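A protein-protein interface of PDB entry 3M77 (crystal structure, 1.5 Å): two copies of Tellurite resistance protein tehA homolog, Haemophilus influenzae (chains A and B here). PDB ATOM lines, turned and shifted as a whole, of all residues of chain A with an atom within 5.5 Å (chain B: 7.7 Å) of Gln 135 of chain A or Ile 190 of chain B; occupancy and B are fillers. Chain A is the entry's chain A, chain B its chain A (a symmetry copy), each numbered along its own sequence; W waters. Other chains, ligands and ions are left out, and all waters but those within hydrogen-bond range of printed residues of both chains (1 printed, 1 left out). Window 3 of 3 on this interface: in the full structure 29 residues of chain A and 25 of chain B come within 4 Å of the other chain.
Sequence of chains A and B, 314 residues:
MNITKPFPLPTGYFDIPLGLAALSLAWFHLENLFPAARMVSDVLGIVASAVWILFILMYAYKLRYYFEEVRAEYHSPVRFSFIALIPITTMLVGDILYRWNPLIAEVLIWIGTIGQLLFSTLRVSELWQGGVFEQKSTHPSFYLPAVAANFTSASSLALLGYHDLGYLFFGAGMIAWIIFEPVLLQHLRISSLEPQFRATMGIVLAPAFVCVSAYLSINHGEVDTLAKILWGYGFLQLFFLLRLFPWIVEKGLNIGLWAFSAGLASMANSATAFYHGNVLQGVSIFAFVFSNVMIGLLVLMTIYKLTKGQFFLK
2 positions are printed for both chains.
O of Leu 127 of chain A touches O of Leu 188 of chain B, 3.7 Å away.
O of Arg 189 of chain B touches CA of Gly 130 of chain A, 3.3 Å away.
Ile 190 of chain B touches Gly 130 of chain A.
Ser 191 of chain B touches Gly 130 of chain A.
Gly 131 of chain A touches Ser 192 of chain B (N to OG, 3.7 Å).
Phe 133 of chain A touches Gln 186 of chain B (CE2 to OE1, 3.6 Å).
CA of Ile 190 of chain B touches O of Phe 133 of chain A, 3.6 Å away.
Gln 135 of chain A touches Ile 190 of chain B.
Val 183 of chain A touches Gln 186 of chain B (CG2 to OE1, 3.8 Å).
Arg 189 of chain B touches Val 183 of chain A.
Water W1 lies within hydrogen-bond range of O of Phe 133 of chain A (2.7 Å) and O of Ile 190 of chain B (2.8 Å).
Hydrophobic or aromatic side chains of chain A that line the printed part of chain B: Leu 127, Phe 133 and Val 183.
Among the printed residues, 18 pairs touch across the chains.
Among the printed residues, no Asp or Glu carboxylate lies within 4 Å of a Lys or Arg side-chain nitrogen of the other chain.
The side-chain amide oxygen (OE1) of Gln 186 of chain B lies within hydrogen-bond range of the guanidinium group (NH2) of Arg 189 of chain B (2.8 Å).
The side-chain hydroxyl of Thr 138 of chain A sits at hydrogen-bond distance from the backbone carbonyl oxygen of Gln 135 of chain A (2.8 Å).
The side-chain amide nitrogen of Gln 135 of chain A sits at hydrogen-bond distance from a ring nitrogen (ND1) of His 187 of chain A (3.1 Å).
Of chain B, only Gln 186 and Ile 190 come within 4 Å of Gln 135 of chain A.
Printed residues of chain B within 4 Å of Thr 138 of chain A: Gln 186 (2.9 Å).
Printed residues of chain A within 4 Å of Arg 189 of chain B: Leu 127, Gly 130, Gly 131, Phe 133 and Val 183.
Of the printed residues of chain A, Ile 190 of chain B touches Gly 130, Gly 131, Phe 133 and Gln 135.
Printed residues of chain A within 4 Å of Ser 192 of chain B: Gly 130 (3.1 Å) and Gly 131 (3.7 Å).
The nearest residue of chain B that does not touch Gln 135 of chain A is His 187 of chain B (7.3 Å).
The nearest printed residue of chain A that does not touch Ile 190 of chain B is Glu 134 of chain A (4.1 Å).
The nearest printed residue of chain A that does not touch Leu 188 of chain B is Gly 131 of chain A (5.3 Å).
O of Gly 130 of chain A lies close to OG of Ser 192 of chain B.
The backbone carbonyl oxygen (O) of Leu 127 of chain A sits close to the backbone carbonyl oxygen (O) of Arg 189 of chain B, at 3.4 Å.
The backbone NH (N) of Gly 130 of chain A sits close to the backbone carbonyl oxygen (O) of Leu 188 of chain B, 3.5 Å away.
The backbone carbonyl oxygen (O) of Ile 190 of chain B sits at hydrogen-bond distance from the backbone NH (N) of Gly 131 of chain A (3.0 Å).
O of Phe 133 of chain A lies close to O of Arg 189 of chain B.
OG1 of Thr 138 of chain A sits at hydrogen-bond distance from NE2 of Gln 186 of chain B, 2.9 Å away.
The side-chain amide oxygen (OE1) of Gln 135 of chain A sits at hydrogen-bond distance from the side-chain amide nitrogen (NE2) of Gln 186 of chain B (3.3 Å).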
ATOM      1  N   LEU A 127       4.587 -13.953  25.404  1.00  0.00           N
ATOM      2  CA  LEU A 127       4.873 -14.479  24.060  1.00  0.00           C
ATOM      3  C   LEU A 127       6.172 -15.311  24.058  1.00  0.00           C
ATOM      4  O   LEU A 127       6.294 -16.266  23.282  1.00  0.00           O
ATOM      5  CB  LEU A 127       4.906 -13.379  22.996  1.00  0.00           C
ATOM      6  CG  LEU A 127       3.678 -12.508  22.810  1.00  0.00           C
ATOM      7  CD1 LEU A 127       3.926 -11.398  21.842  1.00  0.00           C
ATOM      8  CD2 LEU A 127       2.503 -13.346  22.311  1.00  0.00           C
ATOM      9  N   GLY A 130       6.580 -19.207  24.008  1.00  0.00           N
ATOM     10  CA  GLY A 130       6.524 -19.961  22.762  1.00  0.00           C
ATOM     11  C   GLY A 130       5.209 -20.675  22.529  1.00  0.00           C
ATOM     12  O   GLY A 130       4.400 -20.830  23.427  1.00  0.00           O
ATOM     13  N   GLY A 131       4.999 -21.086  21.279  1.00  0.00           N
ATOM     14  CA  GLY A 131       3.930 -22.003  20.946  1.00  0.00           C
ATOM     15  C   GLY A 131       2.575 -21.388  20.686  1.00  0.00           C
ATOM     16  O   GLY A 131       1.626 -22.117  20.350  1.00  0.00           O
ATOM     17  N   VAL A 132       2.457 -20.073  20.849  1.00  0.00           N
ATOM     18  CA  VAL A 132       1.215 -19.361  20.650  1.00  0.00           C
ATOM     19  C   VAL A 132       1.356 -18.382  19.470  1.00  0.00           C
ATOM     20  O   VAL A 132       0.680 -18.506  18.430  1.00  0.00           O
ATOM     21  CB  VAL A 132       0.724 -18.626  21.916  1.00  0.00           C
ATOM     22  CG1 VAL A 132      -0.581 -17.921  21.610  1.00  0.00           C
ATOM     23  CG2 VAL A 132       0.481 -19.605  23.069  1.00  0.00           C
ATOM     24  N   PHE A 133       2.309 -17.471  19.600  1.00  0.00           N
ATOM     25  CA  PHE A 133       2.709 -16.593  18.517  1.00  0.00           C
ATOM     26  C   PHE A 133       3.310 -17.524  17.458  1.00  0.00           C
ATOM     27  O   PHE A 133       4.075 -18.464  17.784  1.00  0.00           O
ATOM     28  CB  PHE A 133       3.769 -15.655  19.053  1.00  0.00           C
ATOM     29  CG  PHE A 133       4.236 -14.566  18.102  1.00  0.00           C
ATOM     30  CD1 PHE A 133       3.737 -13.280  18.184  1.00  0.00           C
ATOM     31  CD2 PHE A 133       5.247 -14.834  17.162  1.00  0.00           C
ATOM     32  CE1 PHE A 133       4.211 -12.272  17.355  1.00  0.00           C
ATOM     33  CE2 PHE A 133       5.700 -13.836  16.332  1.00  0.00           C
ATOM     34  CZ  PHE A 133       5.186 -12.548  16.441  1.00  0.00           C
ATOM     35  N   GLU A 134       2.977 -17.262  16.207  1.00  0.00           N
ATOM     36  CA  GLU A 134       3.466 -18.023  15.074  1.00  0.00           C
ATOM     37  C   GLU A 134       4.153 -17.040  14.101  1.00  0.00           C
ATOM     38  O   GLU A 134       4.020 -15.823  14.236  1.00  0.00           O
ATOM     39  CB  GLU A 134       2.288 -18.682  14.342  1.00  0.00           C
ATOM     40  CG  GLU A 134       1.614 -19.796  15.167  1.00  0.00           C
ATOM     41  CD  GLU A 134       0.569 -20.567  14.359  1.00  0.00           C
ATOM     42  OE1 GLU A 134      -0.514 -20.046  14.206  1.00  0.00           O
ATOM     43  OE2 GLU A 134       0.869 -21.658  13.852  1.00  0.00           O
ATOM     44  N   GLN A 135       4.855 -17.562  13.103  1.00  0.00           N
ATOM     45  CA  GLN A 135       5.522 -16.674  12.134  1.00  0.00           C
ATOM     46  C   GLN A 135       4.478 -15.724  11.515  1.00  0.00           C
ATOM     47  O   GLN A 135       4.754 -14.543  11.329  1.00  0.00           O
ATOM     48  CB  GLN A 135       6.214 -17.477  11.038  1.00  0.00           C
ATOM     49  CG  GLN A 135       6.954 -16.613  10.041  1.00  0.00           C
ATOM     50  CD  GLN A 135       8.065 -15.783  10.630  1.00  0.00           C
ATOM     51  OE1 GLN A 135       8.841 -16.242  11.507  1.00  0.00           O
ATOM     52  NE2 GLN A 135       8.123 -14.534  10.209  1.00  0.00           N
ATOM     53  N   LYS A 136       3.272 -16.250  11.245  1.00  0.00           N
ATOM     54  CA  LYS A 136       2.239 -15.430  10.643  1.00  0.00           C
ATOM     55  C   LYS A 136       1.667 -14.346  11.569  1.00  0.00           C
ATOM     56  O   LYS A 136       0.937 -13.496  11.099  1.00  0.00           O
ATOM     57  CB  LYS A 136       1.084 -16.289  10.105  1.00  0.00           C
ATOM     58  CG  LYS A 136       0.299 -16.978  11.175  1.00  0.00           C
ATOM     59  CD  LYS A 136      -0.872 -17.786  10.575  1.00  0.00           C
ATOM     60  CE  LYS A 136      -1.843 -18.167  11.655  1.00  0.00           C
ATOM     61  NZ  LYS A 136      -2.902 -19.023  11.073  1.00  0.00           N
ATOM     62  N   SER A 137       2.022 -14.365  12.866  1.00  0.00           N
ATOM     63  CA  SER A 137       1.615 -13.357  13.833  1.00  0.00           C
ATOM     64  C   SER A 137       2.490 -12.096  13.758  1.00  0.00           C
ATOM     65  O   SER A 137       2.254 -11.143  14.486  1.00  0.00           O
ATOM     66  CB  SER A 137       1.770 -13.897  15.240  1.00  0.00           C
ATOM     67  OG  SER A 137       1.113 -15.137  15.439  1.00  0.00           O
ATOM     68  N   THR A 138       3.513 -12.110  12.898  1.00  0.00           N
ATOM     69  CA  THR A 138       4.521 -11.048  12.835  1.00  0.00           C
ATOM     70  C   THR A 138       3.929  -9.888  12.035  1.00  0.00           C
ATOM     71  O   THR A 138       4.087  -9.808  10.821  1.00  0.00           O
ATOM     72  CB  THR A 138       5.821 -11.560  12.239  1.00  0.00           C
ATOM     73  OG1 THR A 138       6.222 -12.790  12.859  1.00  0.00           O
ATOM     74  CG2 THR A 138       6.948 -10.536  12.398  1.00  0.00           C
ATOM     75  N   VAL A 183      12.692  -8.448  11.923  1.00  0.00           N
ATOM     76  CA  VAL A 183      11.934  -9.674  11.666  1.00  0.00           C
ATOM     77  C   VAL A 183      10.601  -9.347  11.005  1.00  0.00           C
ATOM     78  O   VAL A 183      10.104 -10.135  10.193  1.00  0.00           O
ATOM     79  CB  VAL A 183      11.791 -10.588  12.904  1.00  0.00           C
ATOM     80  CG1 VAL A 183      13.210 -10.977  13.361  1.00  0.00           C
ATOM     81  CG2 VAL A 183      10.998  -9.934  14.003  1.00  0.00           C
ATOM     82  N   HIS A 187       9.587 -10.825   7.292  1.00  0.00           N
ATOM     83  CA  HIS A 187       8.312 -11.481   7.139  1.00  0.00           C
ATOM     84  C   HIS A 187       7.482 -10.876   6.024  1.00  0.00           C
ATOM     85  O   HIS A 187       6.899 -11.599   5.223  1.00  0.00           O
ATOM     86  CB  HIS A 187       7.550 -11.452   8.446  1.00  0.00           C
ATOM     87  CG  HIS A 187       6.207 -12.098   8.365  1.00  0.00           C
ATOM     88  ND1 HIS A 187       6.057 -13.462   8.188  1.00  0.00           N
ATOM     89  CD2 HIS A 187       4.955 -11.570   8.390  1.00  0.00           C
ATOM     90  CE1 HIS A 187       4.763 -13.740   8.119  1.00  0.00           C
ATOM     91  NE2 HIS A 187       4.073 -12.615   8.266  1.00  0.00           N
ATOM     92  N   GLN B 135      17.941 -23.419  13.393  1.00  0.00           N
ATOM     93  CA  GLN B 135      17.033 -22.439  14.015  1.00  0.00           C
ATOM     94  C   GLN B 135      16.950 -22.715  15.529  1.00  0.00           C
ATOM     95  O   GLN B 135      16.948 -21.781  16.325  1.00  0.00           O
ATOM     96  CB  GLN B 135      15.642 -22.505  13.394  1.00  0.00           C
ATOM     97  CG  GLN B 135      14.682 -21.486  13.966  1.00  0.00           C
ATOM     98  CD  GLN B 135      15.094 -20.051  13.765  1.00  0.00           C
ATOM     99  OE1 GLN B 135      15.598 -19.654  12.683  1.00  0.00           O
ATOM    100  NE2 GLN B 135      14.948 -19.266  14.815  1.00  0.00           N
ATOM    101  N   LEU B 184      16.764 -13.691  18.148  1.00  0.00           N
ATOM    102  CA  LEU B 184      16.527 -14.429  19.388  1.00  0.00           C
ATOM    103  C   LEU B 184      15.093 -14.269  19.900  1.00  0.00           C
ATOM    104  O   LEU B 184      14.404 -15.249  20.215  1.00  0.00           O
ATOM    105  CB  LEU B 184      17.493 -14.022  20.489  1.00  0.00           C
ATOM    106  CG  LEU B 184      17.249 -14.670  21.849  1.00  0.00           C
ATOM    107  CD1 LEU B 184      17.496 -16.173  21.812  1.00  0.00           C
ATOM    108  CD2 LEU B 184      18.164 -14.057  22.882  1.00  0.00           C
ATOM    109  N   LEU B 185      14.618 -13.022  19.979  1.00  0.00           N
ATOM    110  CA  LEU B 185      13.288 -12.826  20.549  1.00  0.00           C
ATOM    111  C   LEU B 185      12.200 -13.434  19.652  1.00  0.00           C
ATOM    112  O   LEU B 185      11.180 -13.949  20.134  1.00  0.00           O
ATOM    113  CB  LEU B 185      12.974 -11.379  20.884  1.00  0.00           C
ATOM    114  CG  LEU B 185      13.944 -10.728  21.879  1.00  0.00           C
ATOM    115  CD1 LEU B 185      13.477  -9.331  22.321  1.00  0.00           C
ATOM    116  CD2 LEU B 185      14.241 -11.574  23.068  1.00  0.00           C
ATOM    117  N   GLN B 186      12.386 -13.331  18.337  1.00  0.00           N
ATOM    118  CA  GLN B 186      11.450 -13.975  17.425  1.00  0.00           C
ATOM    119  C   GLN B 186      11.422 -15.492  17.642  1.00  0.00           C
ATOM    120  O   GLN B 186      10.363 -16.093  17.639  1.00  0.00           O
ATOM    121  CB  GLN B 186      11.759 -13.592  15.981  1.00  0.00           C
ATOM    122  CG  GLN B 186      10.836 -14.192  14.926  1.00  0.00           C
ATOM    123  CD  GLN B 186       9.499 -13.488  14.799  1.00  0.00           C
ATOM    124  OE1 GLN B 186       9.093 -12.709  15.691  1.00  0.00           O
ATOM    125  NE2 GLN B 186       8.766 -13.786  13.688  1.00  0.00           N
ATOM    126  N   HIS B 187      12.589 -16.091  17.775  1.00  0.00           N
ATOM    127  CA  HIS B 187      12.668 -17.504  18.051  1.00  0.00           C
ATOM    128  C   HIS B 187      11.988 -17.875  19.354  1.00  0.00           C
ATOM    129  O   HIS B 187      11.250 -18.854  19.411  1.00  0.00           O
ATOM    130  CB  HIS B 187      14.113 -17.954  18.057  1.00  0.00           C
ATOM    131  CG  HIS B 187      14.280 -19.408  18.356  1.00  0.00           C
ATOM    132  ND1 HIS B 187      13.869 -20.391  17.474  1.00  0.00           N
ATOM    133  CD2 HIS B 187      14.770 -20.046  19.450  1.00  0.00           C
ATOM    134  CE1 HIS B 187      14.112 -21.575  18.019  1.00  0.00           C
ATOM    135  NE2 HIS B 187      14.683 -21.395  19.204  1.00  0.00           N
ATOM    136  N   LEU B 188      12.210 -17.103  20.401  1.00  0.00           N
ATOM    137  CA  LEU B 188      11.568 -17.410  21.673  1.00  0.00           C
ATOM    138  C   LEU B 188      10.040 -17.309  21.550  1.00  0.00           C
ATOM    139  O   LEU B 188       9.303 -18.112  22.138  1.00  0.00           O
ATOM    140  CB  LEU B 188      12.053 -16.472  22.783  1.00  0.00           C
ATOM    141  CG  LEU B 188      13.514 -16.612  23.162  1.00  0.00           C
ATOM    142  CD1 LEU B 188      13.840 -15.591  24.212  1.00  0.00           C
ATOM    143  CD2 LEU B 188      13.821 -18.005  23.681  1.00  0.00           C
ATOM    144  N   ARG B 189       9.566 -16.295  20.816  1.00  0.00           N
ATOM    145  CA  ARG B 189       8.133 -16.151  20.609  1.00  0.00           C
ATOM    146  C   ARG B 189       7.511 -17.398  19.959  1.00  0.00           C
ATOM    147  O   ARG B 189       6.392 -17.821  20.305  1.00  0.00           O
ATOM    148  CB  ARG B 189       7.811 -14.912  19.765  1.00  0.00           C
ATOM    149  CG  ARG B 189       7.841 -13.590  20.510  1.00  0.00           C
ATOM    150  CD  ARG B 189       7.261 -12.483  19.655  1.00  0.00           C
ATOM    151  NE  ARG B 189       8.156 -12.061  18.559  1.00  0.00           N
ATOM    152  CZ  ARG B 189       9.084 -11.122  18.673  1.00  0.00           C
ATOM    153  NH1 ARG B 189       9.242 -10.480  19.820  1.00  0.00           N
ATOM    154  NH2 ARG B 189       9.836 -10.793  17.638  1.00  0.00           N
ATOM    155  N   ILE B 190       8.180 -17.941  18.957  1.00  0.00           N
ATOM    156  CA  ILE B 190       7.635 -19.043  18.166  1.00  0.00           C
ATOM    157  C   ILE B 190       7.877 -20.397  18.817  1.00  0.00           C
ATOM    158  O   ILE B 190       6.946 -21.200  18.968  1.00  0.00           O
ATOM    159  CB  ILE B 190       8.239 -19.000  16.746  1.00  0.00           C
ATOM    160  CG1 ILE B 190       7.736 -17.751  16.039  1.00  0.00           C
ATOM    161  CG2 ILE B 190       7.864 -20.268  15.967  1.00  0.00           C
ATOM    162  CD1 ILE B 190       8.374 -17.527  14.708  1.00  0.00           C
ATOM    163  N   SER B 191       9.098 -20.620  19.265  1.00  0.00           N
ATOM    164  CA  SER B 191       9.536 -21.922  19.789  1.00  0.00           C
ATOM    165  C   SER B 191       9.673 -21.917  21.312  1.00  0.00           C
ATOM    166  O   SER B 191      10.405 -21.111  21.851  1.00  0.00           O
ATOM    167  CB  SER B 191      10.885 -22.263  19.156  1.00  0.00           C
ATOM    168  OG  SER B 191      10.773 -22.480  17.743  1.00  0.00           O
ATOM    169  N   SER B 192       8.936 -22.777  22.021  1.00  0.00           N
ATOM    170  CA  SER B 192       9.039 -22.788  23.482  1.00  0.00           C
ATOM    171  C   SER B 192      10.377 -23.400  23.873  1.00  0.00           C
ATOM    172  O   SER B 192      10.579 -24.629  23.687  1.00  0.00           O
ATOM    173  CB  SER B 192       7.917 -23.629  24.135  1.00  0.00           C
ATOM    174  OG  SER B 192       6.622 -23.129  23.863  1.00  0.00           O
ATOM    175  N   LEU B 193      11.231 -22.591  24.510  1.00  0.00           N
ATOM    176  CA  LEU B 193      12.550 -23.026  24.980  1.00  0.00           C
ATOM    177  C   LEU B 193      12.365 -24.115  26.029  1.00  0.00           C
ATOM    178  O   LEU B 193      11.659 -23.898  27.036  1.00  0.00           O
ATOM    179  CB  LEU B 193      13.283 -21.844  25.606  1.00  0.00           C
ATOM    180  CG  LEU B 193      14.712 -21.430  25.216  1.00  0.00           C
ATOM    181  CD1 LEU B 193      15.363 -20.598  26.326  1.00  0.00           C
ATOM    182  CD2 LEU B 193      15.583 -22.609  24.792  1.00  0.00           C
HETATM  183  O   HOH W   1       4.494 -21.112  17.644  1.00  0.00           O
